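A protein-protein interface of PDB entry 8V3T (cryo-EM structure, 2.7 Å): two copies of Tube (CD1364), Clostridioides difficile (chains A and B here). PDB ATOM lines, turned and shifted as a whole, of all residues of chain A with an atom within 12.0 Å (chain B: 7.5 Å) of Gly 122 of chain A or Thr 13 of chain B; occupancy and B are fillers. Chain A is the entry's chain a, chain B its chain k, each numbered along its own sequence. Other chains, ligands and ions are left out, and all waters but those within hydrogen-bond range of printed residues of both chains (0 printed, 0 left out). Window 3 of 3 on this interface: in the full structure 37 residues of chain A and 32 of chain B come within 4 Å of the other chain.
The backbone NH (N) of Gly 12 of chain B sits at hydrogen-bond distance from the backbone carbonyl oxygen (O) of Val 123 of chain A, 3.0 Å away.
N of Gly 125 of chain A sits at hydrogen-bond distance from O of Met 10 of chain B (3.1 Å).
N of Val 121 of chain A lies within hydrogen-bond range of O of Lys 28 of chain B, 3.1 Å away.
The side-chain hydroxyl of Thr 13 of chain B is in hydrogen-bond range of the backbone NH of Gly 122 of chain A (3.0 Å).
The side-chain carboxylate (OE2) of Glu 120 of chain A is in salt-bridge range of the side-chain amino group (NZ) of Lys 28 of chain B, at 3.98 Å.
O of His 66 of chain A lies close to N of Met 10 of chain B (3.4 Å).
The backbone NH (N) of His 66 of chain A is in hydrogen-bond range of the backbone carbonyl oxygen (O) of Gly 125 of chain A.
Gly 12 of chain B touches Trp 119 of chain A.
Trp 119 of chain A touches Gly 15 of chain B (CH2 to C, 3.7 Å).
Trp 119 of chain A touches Glu 16 of chain B (CH2 to N, 3.8 Å).
Trp 119 of chain A touches Val 27 of chain B.
Glu 120 of chain A touches Gly 12 of chain B.
Glu 120 of chain A touches Thr 13 of chain B.
Val 121 of chain A touches Gly 12 of chain B.
Thr 13 of chain B touches Val 121 of chain A.
CG1 of Val 121 of chain A touches O of Val 27 of chain B, 3.8 Å away.
O of Met 10 of chain B touches CA of Lys 124 of chain A (3.8 Å).
Gly 122 of chain A touches just one residue of chain B: Thr 13.
Of the printed residues of chain A, Thr 13 of chain B touches Glu 120 (3.9 Å), Val 121 (3.98 Å) and Gly 122 (3.0 Å).
Of chain A, only Trp 119 comes within 4 Å of Gly 15 of chain B.
Printed residues of chain B within 4 Å of Val 121 of chain A: Gly 12, Thr 13, Val 27 and Lys 28.
Printed residues of chain B within 4 Å of Lys 124 of chain A: Met 10 (3.8 Å).
Of the printed residues of chain A, Lys 28 of chain B touches Glu 120 and Val 121.
Of the printed residues of chain A, Val 27 of chain B touches Trp 119 (3.8 Å) and Val 121 (3.8 Å).
Glu 126 of chain A touches none of the printed residues of chain B.
The nearest printed residue of chain A that does not touch Thr 13 of chain B is Val 123 of chain A (5.0 Å).
Of the 12 printed residues of chain B, 7 touch a printed residue of chain A.
Printed residues of chain B that touch a printed residue of chain A: Met 10, Gly 12, Thr 13, Gly 15, Glu 16, Val 27 and Lys 28.
Hydrophobic or aromatic side chains of chain B that line the printed part of chain A: Met 10 and Val 27.
Of the 10 printed residues of chain A, 8 touch a printed residue of chain B.
Among the printed residues, Asp or Glu carboxylates within 4 Å of a Lys or Arg side-chain nitrogen of the other chain: Glu 120 of chain A with Lys 28 of chain B.
No position is printed for both chains.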
ATOM      1  N   HIS A  66      16.709   8.477  28.417  1.00  0.00           N
ATOM      2  CA  HIS A  66      16.084   7.546  29.353  1.00  0.00           C
ATOM      3  C   HIS A  66      17.059   6.410  29.627  1.00  0.00           C
ATOM      4  O   HIS A  66      17.173   5.468  28.842  1.00  0.00           O
ATOM      5  CB  HIS A  66      14.759   7.034  28.802  1.00  0.00           C
ATOM      6  CG  HIS A  66      13.985   6.203  29.775  1.00  0.00           C
ATOM      7  ND1 HIS A  66      14.073   6.380  31.138  1.00  0.00           N
ATOM      8  CD2 HIS A  66      13.100   5.198  29.583  1.00  0.00           C
ATOM      9  CE1 HIS A  66      13.280   5.516  31.744  1.00  0.00           C
ATOM     10  NE2 HIS A  66      12.679   4.785  30.823  1.00  0.00           N
ATOM     11  N   ASP A 118       6.790   5.930  28.756  1.00  0.00           N
ATOM     12  CA  ASP A 118       6.575   6.520  27.437  1.00  0.00           C
ATOM     13  C   ASP A 118       7.562   5.854  26.481  1.00  0.00           C
ATOM     14  O   ASP A 118       8.739   6.219  26.458  1.00  0.00           O
ATOM     15  CB  ASP A 118       6.760   8.028  27.478  1.00  0.00           C
ATOM     16  CG  ASP A 118       6.270   8.713  26.218  1.00  0.00           C
ATOM     17  OD1 ASP A 118       5.871   8.009  25.267  1.00  0.00           O
ATOM     18  OD2 ASP A 118       6.286   9.961  26.178  1.00  0.00           O
ATOM     19  N   TRP A 119       7.078   4.889  25.702  1.00  0.00           N
ATOM     20  CA  TRP A 119       7.929   4.187  24.752  1.00  0.00           C
ATOM     21  C   TRP A 119       7.148   3.873  23.485  1.00  0.00           C
ATOM     22  O   TRP A 119       5.916   3.842  23.475  1.00  0.00           O
ATOM     23  CB  TRP A 119       8.529   2.907  25.360  1.00  0.00           C
ATOM     24  CG  TRP A 119       7.548   1.979  26.018  1.00  0.00           C
ATOM     25  CD1 TRP A 119       7.178   1.985  27.329  1.00  0.00           C
ATOM     26  CD2 TRP A 119       6.845   0.888  25.409  1.00  0.00           C
ATOM     27  NE1 TRP A 119       6.276   0.982  27.573  1.00  0.00           N
ATOM     28  CE2 TRP A 119       6.054   0.293  26.411  1.00  0.00           C
ATOM     29  CE3 TRP A 119       6.798   0.365  24.113  1.00  0.00           C
ATOM     30  CZ2 TRP A 119       5.229  -0.801  26.159  1.00  0.00           C
ATOM     31  CZ3 TRP A 119       5.977  -0.721  23.867  1.00  0.00           C
ATOM     32  CH2 TRP A 119       5.204  -1.291  24.885  1.00  0.00           C
ATOM     33  N   GLU A 120       7.895   3.646  22.408  1.00  0.00           N
ATOM     34  CA  GLU A 120       7.341   3.351  21.096  1.00  0.00           C
ATOM     35  C   GLU A 120       8.279   2.386  20.390  1.00  0.00           C
ATOM     36  O   GLU A 120       9.493   2.435  20.588  1.00  0.00           O
ATOM     37  CB  GLU A 120       7.179   4.618  20.252  1.00  0.00           C
ATOM     38  CG  GLU A 120       6.319   4.443  19.019  1.00  0.00           C
ATOM     39  CD  GLU A 120       6.010   5.758  18.332  1.00  0.00           C
ATOM     40  OE1 GLU A 120       5.801   6.766  19.034  1.00  0.00           O
ATOM     41  OE2 GLU A 120       5.982   5.782  17.084  1.00  0.00           O
ATOM     42  N   VAL A 121       7.716   1.528  19.542  1.00  0.00           N
ATOM     43  CA  VAL A 121       8.541   0.574  18.813  1.00  0.00           C
ATOM     44  C   VAL A 121       9.377   1.320  17.780  1.00  0.00           C
ATOM     45  O   VAL A 121       8.869   2.168  17.035  1.00  0.00           O
ATOM     46  CB  VAL A 121       7.675  -0.519  18.167  1.00  0.00           C
ATOM     47  CG1 VAL A 121       7.032  -1.381  19.237  1.00  0.00           C
ATOM     48  CG2 VAL A 121       6.608   0.086  17.270  1.00  0.00           C
ATOM     49  N   GLY A 122      10.675   1.029  17.754  1.00  0.00           N
ATOM     50  CA  GLY A 122      11.577   1.695  16.840  1.00  0.00           C
ATOM     51  C   GLY A 122      11.954   3.111  17.213  1.00  0.00           C
ATOM     52  O   GLY A 122      12.503   3.827  16.370  1.00  0.00           O
ATOM     53  N   VAL A 123      11.678   3.541  18.442  1.00  0.00           N
ATOM     54  CA  VAL A 123      11.986   4.890  18.903  1.00  0.00           C
ATOM     55  C   VAL A 123      12.767   4.790  20.206  1.00  0.00           C
ATOM     56  O   VAL A 123      12.386   4.032  21.104  1.00  0.00           O
ATOM     57  CB  VAL A 123      10.709   5.731  19.103  1.00  0.00           C
ATOM     58  CG1 VAL A 123      11.060   7.133  19.566  1.00  0.00           C
ATOM     59  CG2 VAL A 123       9.893   5.781  17.824  1.00  0.00           C
ATOM     60  N   LYS A 124      13.857   5.545  20.308  1.00  0.00           N
ATOM     61  CA  LYS A 124      14.636   5.578  21.537  1.00  0.00           C
ATOM     62  C   LYS A 124      13.958   6.463  22.578  1.00  0.00           C
ATOM     63  O   LYS A 124      13.224   7.397  22.248  1.00  0.00           O
ATOM     64  CB  LYS A 124      16.058   6.068  21.260  1.00  0.00           C
ATOM     65  CG  LYS A 124      16.167   7.550  20.977  1.00  0.00           C
ATOM     66  CD  LYS A 124      17.584   7.932  20.592  1.00  0.00           C
ATOM     67  CE  LYS A 124      17.700   9.426  20.355  1.00  0.00           C
ATOM     68  NZ  LYS A 124      16.873  10.197  21.320  1.00  0.00           N
ATOM     69  N   GLY A 125      14.212   6.155  23.847  1.00  0.00           N
ATOM     70  CA  GLY A 125      13.483   6.777  24.941  1.00  0.00           C
ATOM     71  C   GLY A 125      14.082   8.103  25.384  1.00  0.00           C
ATOM     72  O   GLY A 125      15.298   8.269  25.433  1.00  0.00           O
ATOM     73  N   GLU A 126      13.198   9.042  25.719  1.00  0.00           N
ATOM     74  CA  GLU A 126      13.592  10.354  26.209  1.00  0.00           C
ATOM     75  C   GLU A 126      12.561  10.829  27.223  1.00  0.00           C
ATOM     76  O   GLU A 126      11.406  10.397  27.209  1.00  0.00           O
ATOM     77  CB  GLU A 126      13.723  11.364  25.066  1.00  0.00           C
ATOM     78  CG  GLU A 126      15.148  11.604  24.615  1.00  0.00           C
ATOM     79  CD  GLU A 126      15.218  12.330  23.288  1.00  0.00           C
ATOM     80  OE1 GLU A 126      14.286  13.100  22.981  1.00  0.00           O
ATOM     81  OE2 GLU A 126      16.205  12.127  22.551  1.00  0.00           O
ATOM     82  N   MET B  10      17.485   3.121  26.375  1.00  0.00           N
ATOM     83  CA  MET B  10      16.516   2.055  26.158  1.00  0.00           C
ATOM     84  C   MET B  10      15.809   2.234  24.822  1.00  0.00           C
ATOM     85  O   MET B  10      15.347   3.330  24.492  1.00  0.00           O
ATOM     86  CB  MET B  10      15.486   2.017  27.285  1.00  0.00           C
ATOM     87  CG  MET B  10      16.016   2.400  28.648  1.00  0.00           C
ATOM     88  SD  MET B  10      14.923   1.833  29.963  1.00  0.00           S
ATOM     89  CE  MET B  10      15.648   2.642  31.382  1.00  0.00           C
ATOM     90  N   SER B  11      15.718   1.150  24.062  1.00  0.00           N
ATOM     91  CA  SER B  11      14.954   1.137  22.826  1.00  0.00           C
ATOM     92  C   SER B  11      13.526   0.700  23.116  1.00  0.00           C
ATOM     93  O   SER B  11      13.293  -0.219  23.904  1.00  0.00           O
ATOM     94  CB  SER B  11      15.595   0.198  21.806  1.00  0.00           C
ATOM     95  OG  SER B  11      14.865   0.190  20.593  1.00  0.00           O
ATOM     96  N   GLY B  12      12.571   1.364  22.472  1.00  0.00           N
ATOM     97  CA  GLY B  12      11.176   1.050  22.700  1.00  0.00           C
ATOM     98  C   GLY B  12      10.694  -0.223  22.047  1.00  0.00           C
ATOM     99  O   GLY B  12       9.564  -0.646  22.304  1.00  0.00           O
ATOM    100  N   THR B  13      11.523  -0.842  21.204  1.00  0.00           N
ATOM    101  CA  THR B  13      11.173  -2.123  20.610  1.00  0.00           C
ATOM    102  C   THR B  13      11.127  -3.235  21.651  1.00  0.00           C
ATOM    103  O   THR B  13      10.467  -4.256  21.430  1.00  0.00           O
ATOM    104  CB  THR B  13      12.172  -2.459  19.498  1.00  0.00           C
ATOM    105  OG1 THR B  13      12.189  -1.394  18.541  1.00  0.00           O
ATOM    106  CG2 THR B  13      11.794  -3.743  18.777  1.00  0.00           C
ATOM    107  N   TRP B  14      11.778  -3.045  22.798  1.00  0.00           N
ATOM    108  CA  TRP B  14      11.832  -4.050  23.850  1.00  0.00           C
ATOM    109  C   TRP B  14      10.756  -3.843  24.910  1.00  0.00           C
ATOM    110  O   TRP B  14      10.964  -4.180  26.079  1.00  0.00           O
ATOM    111  CB  TRP B  14      13.216  -4.062  24.497  1.00  0.00           C
ATOM    112  CG  TRP B  14      14.301  -4.527  23.581  1.00  0.00           C
ATOM    113  CD1 TRP B  14      15.250  -3.757  22.978  1.00  0.00           C
ATOM    114  CD2 TRP B  14      14.534  -5.868  23.139  1.00  0.00           C
ATOM    115  NE1 TRP B  14      16.069  -4.536  22.201  1.00  0.00           N
ATOM    116  CE2 TRP B  14      15.647  -5.837  22.281  1.00  0.00           C
ATOM    117  CE3 TRP B  14      13.911  -7.093  23.391  1.00  0.00           C
ATOM    118  CZ2 TRP B  14      16.153  -6.983  21.674  1.00  0.00           C
ATOM    119  CZ3 TRP B  14      14.414  -8.227  22.788  1.00  0.00           C
ATOM    120  CH2 TRP B  14      15.522  -8.165  21.938  1.00  0.00           C
ATOM    121  N   GLY B  15       9.605  -3.297  24.526  1.00  0.00           N
ATOM    122  CA  GLY B  15       8.513  -3.064  25.449  1.00  0.00           C
ATOM    123  C   GLY B  15       7.456  -4.151  25.378  1.00  0.00           C
ATOM    124  O   GLY B  15       7.235  -4.757  24.334  1.00  0.00           O
ATOM    125  N   GLU B  16       6.801  -4.390  26.513  1.00  0.00           N
ATOM    126  CA  GLU B  16       5.772  -5.412  26.631  1.00  0.00           C
ATOM    127  C   GLU B  16       4.612  -4.865  27.449  1.00  0.00           C
ATOM    128  O   GLU B  16       4.798  -4.008  28.315  1.00  0.00           O
ATOM    129  CB  GLU B  16       6.325  -6.686  27.277  1.00  0.00           C
ATOM    130  CG  GLU B  16       6.737  -7.752  26.283  1.00  0.00           C
ATOM    131  CD  GLU B  16       7.715  -8.745  26.869  1.00  0.00           C
ATOM    132  OE1 GLU B  16       8.862  -8.349  27.155  1.00  0.00           O
ATOM    133  OE2 GLU B  16       7.338  -9.920  27.052  1.00  0.00           O
ATOM    134  N   VAL B  27       1.269  -4.145  20.490  1.00  0.00           N
ATOM    135  CA  VAL B  27       1.356  -2.812  21.063  1.00  0.00           C
ATOM    136  C   VAL B  27       2.343  -2.011  20.227  1.00  0.00           C
ATOM    137  O   VAL B  27       3.413  -2.509  19.864  1.00  0.00           O
ATOM    138  CB  VAL B  27       1.760  -2.856  22.554  1.00  0.00           C
ATOM    139  CG1 VAL B  27       3.074  -3.617  22.747  1.00  0.00           C
ATOM    140  CG2 VAL B  27       1.814  -1.451  23.151  1.00  0.00           C
ATOM    141  N   LYS B  28       1.957  -0.787  19.885  1.00  0.00           N
ATOM    142  CA  LYS B  28       2.816   0.131  19.151  1.00  0.00           C
ATOM    143  C   LYS B  28       3.479   1.141  20.077  1.00  0.00           C
ATOM    144  O   LYS B  28       4.665   1.442  19.921  1.00  0.00           O
ATOM    145  CB  LYS B  28       2.007   0.849  18.064  1.00  0.00           C
ATOM    146  CG  LYS B  28       2.830   1.332  16.884  1.00  0.00           C
ATOM    147  CD  LYS B  28       1.953   1.640  15.684  1.00  0.00           C
ATOM    148  CE  LYS B  28       2.739   2.363  14.612  1.00  0.00           C
ATOM    149  NZ  LYS B  28       3.250   3.664  15.109  1.00  0.00           N
ATOM    150  N   LEU B  93       9.776  -2.636  30.265  1.00  0.00           N
ATOM    151  CA  LEU B  93      10.785  -2.192  29.309  1.00  0.00           C
ATOM    152  C   LEU B  93      12.099  -2.860  29.691  1.00  0.00           C
ATOM    153  O   LEU B  93      12.655  -2.578  30.757  1.00  0.00           O
ATOM    154  CB  LEU B  93      10.906  -0.668  29.317  1.00  0.00           C
ATOM    155  CG  LEU B  93      11.566   0.026  28.125  1.00  0.00           C
ATOM    156  CD1 LEU B  93      10.909  -0.381  26.819  1.00  0.00           C
ATOM    157  CD2 LEU B  93      11.512   1.532  28.305  1.00  0.00           C
ATOM    158  N   ASN B  94      12.596  -3.746  28.825  1.00  0.00           N
ATOM    159  CA  ASN B  94      13.774  -4.564  29.135  1.00  0.00           C
ATOM    160  C   ASN B  94      14.695  -4.583  27.916  1.00  0.00           C
ATOM    161  O   ASN B  94      14.574  -5.449  27.045  1.00  0.00           O
ATOM    162  CB  ASN B  94      13.360  -5.971  29.546  1.00  0.00           C
ATOM    163  CG  ASN B  94      14.383  -6.643  30.433  1.00  0.00           C
ATOM    164  OD1 ASN B  94      15.337  -6.015  30.889  1.00  0.00           O
ATOM    165  ND2 ASN B  94      14.191  -7.931  30.683  1.00  0.00           N
ATOM    166  N   ASP B  95      15.627  -3.637  27.873  1.00  0.00           N
ATOM    167  CA  ASP B  95      16.618  -3.575  26.807  1.00  0.00           C
ATOM    168  C   ASP B  95      17.862  -4.341  27.239  1.00  0.00           C
ATOM    169  O   ASP B  95      18.399  -4.061  28.319  1.00  0.00           O
ATOM    170  CB  ASP B  95      16.961  -2.128  26.491  1.00  0.00           C
ATOM    171  CG  ASP B  95      17.705  -1.962  25.175  1.00  0.00           C
ATOM    172  OD1 ASP B  95      18.388  -2.901  24.729  1.00  0.00           O
ATOM    173  OD2 ASP B  95      17.596  -0.873  24.577  1.00  0.00           O
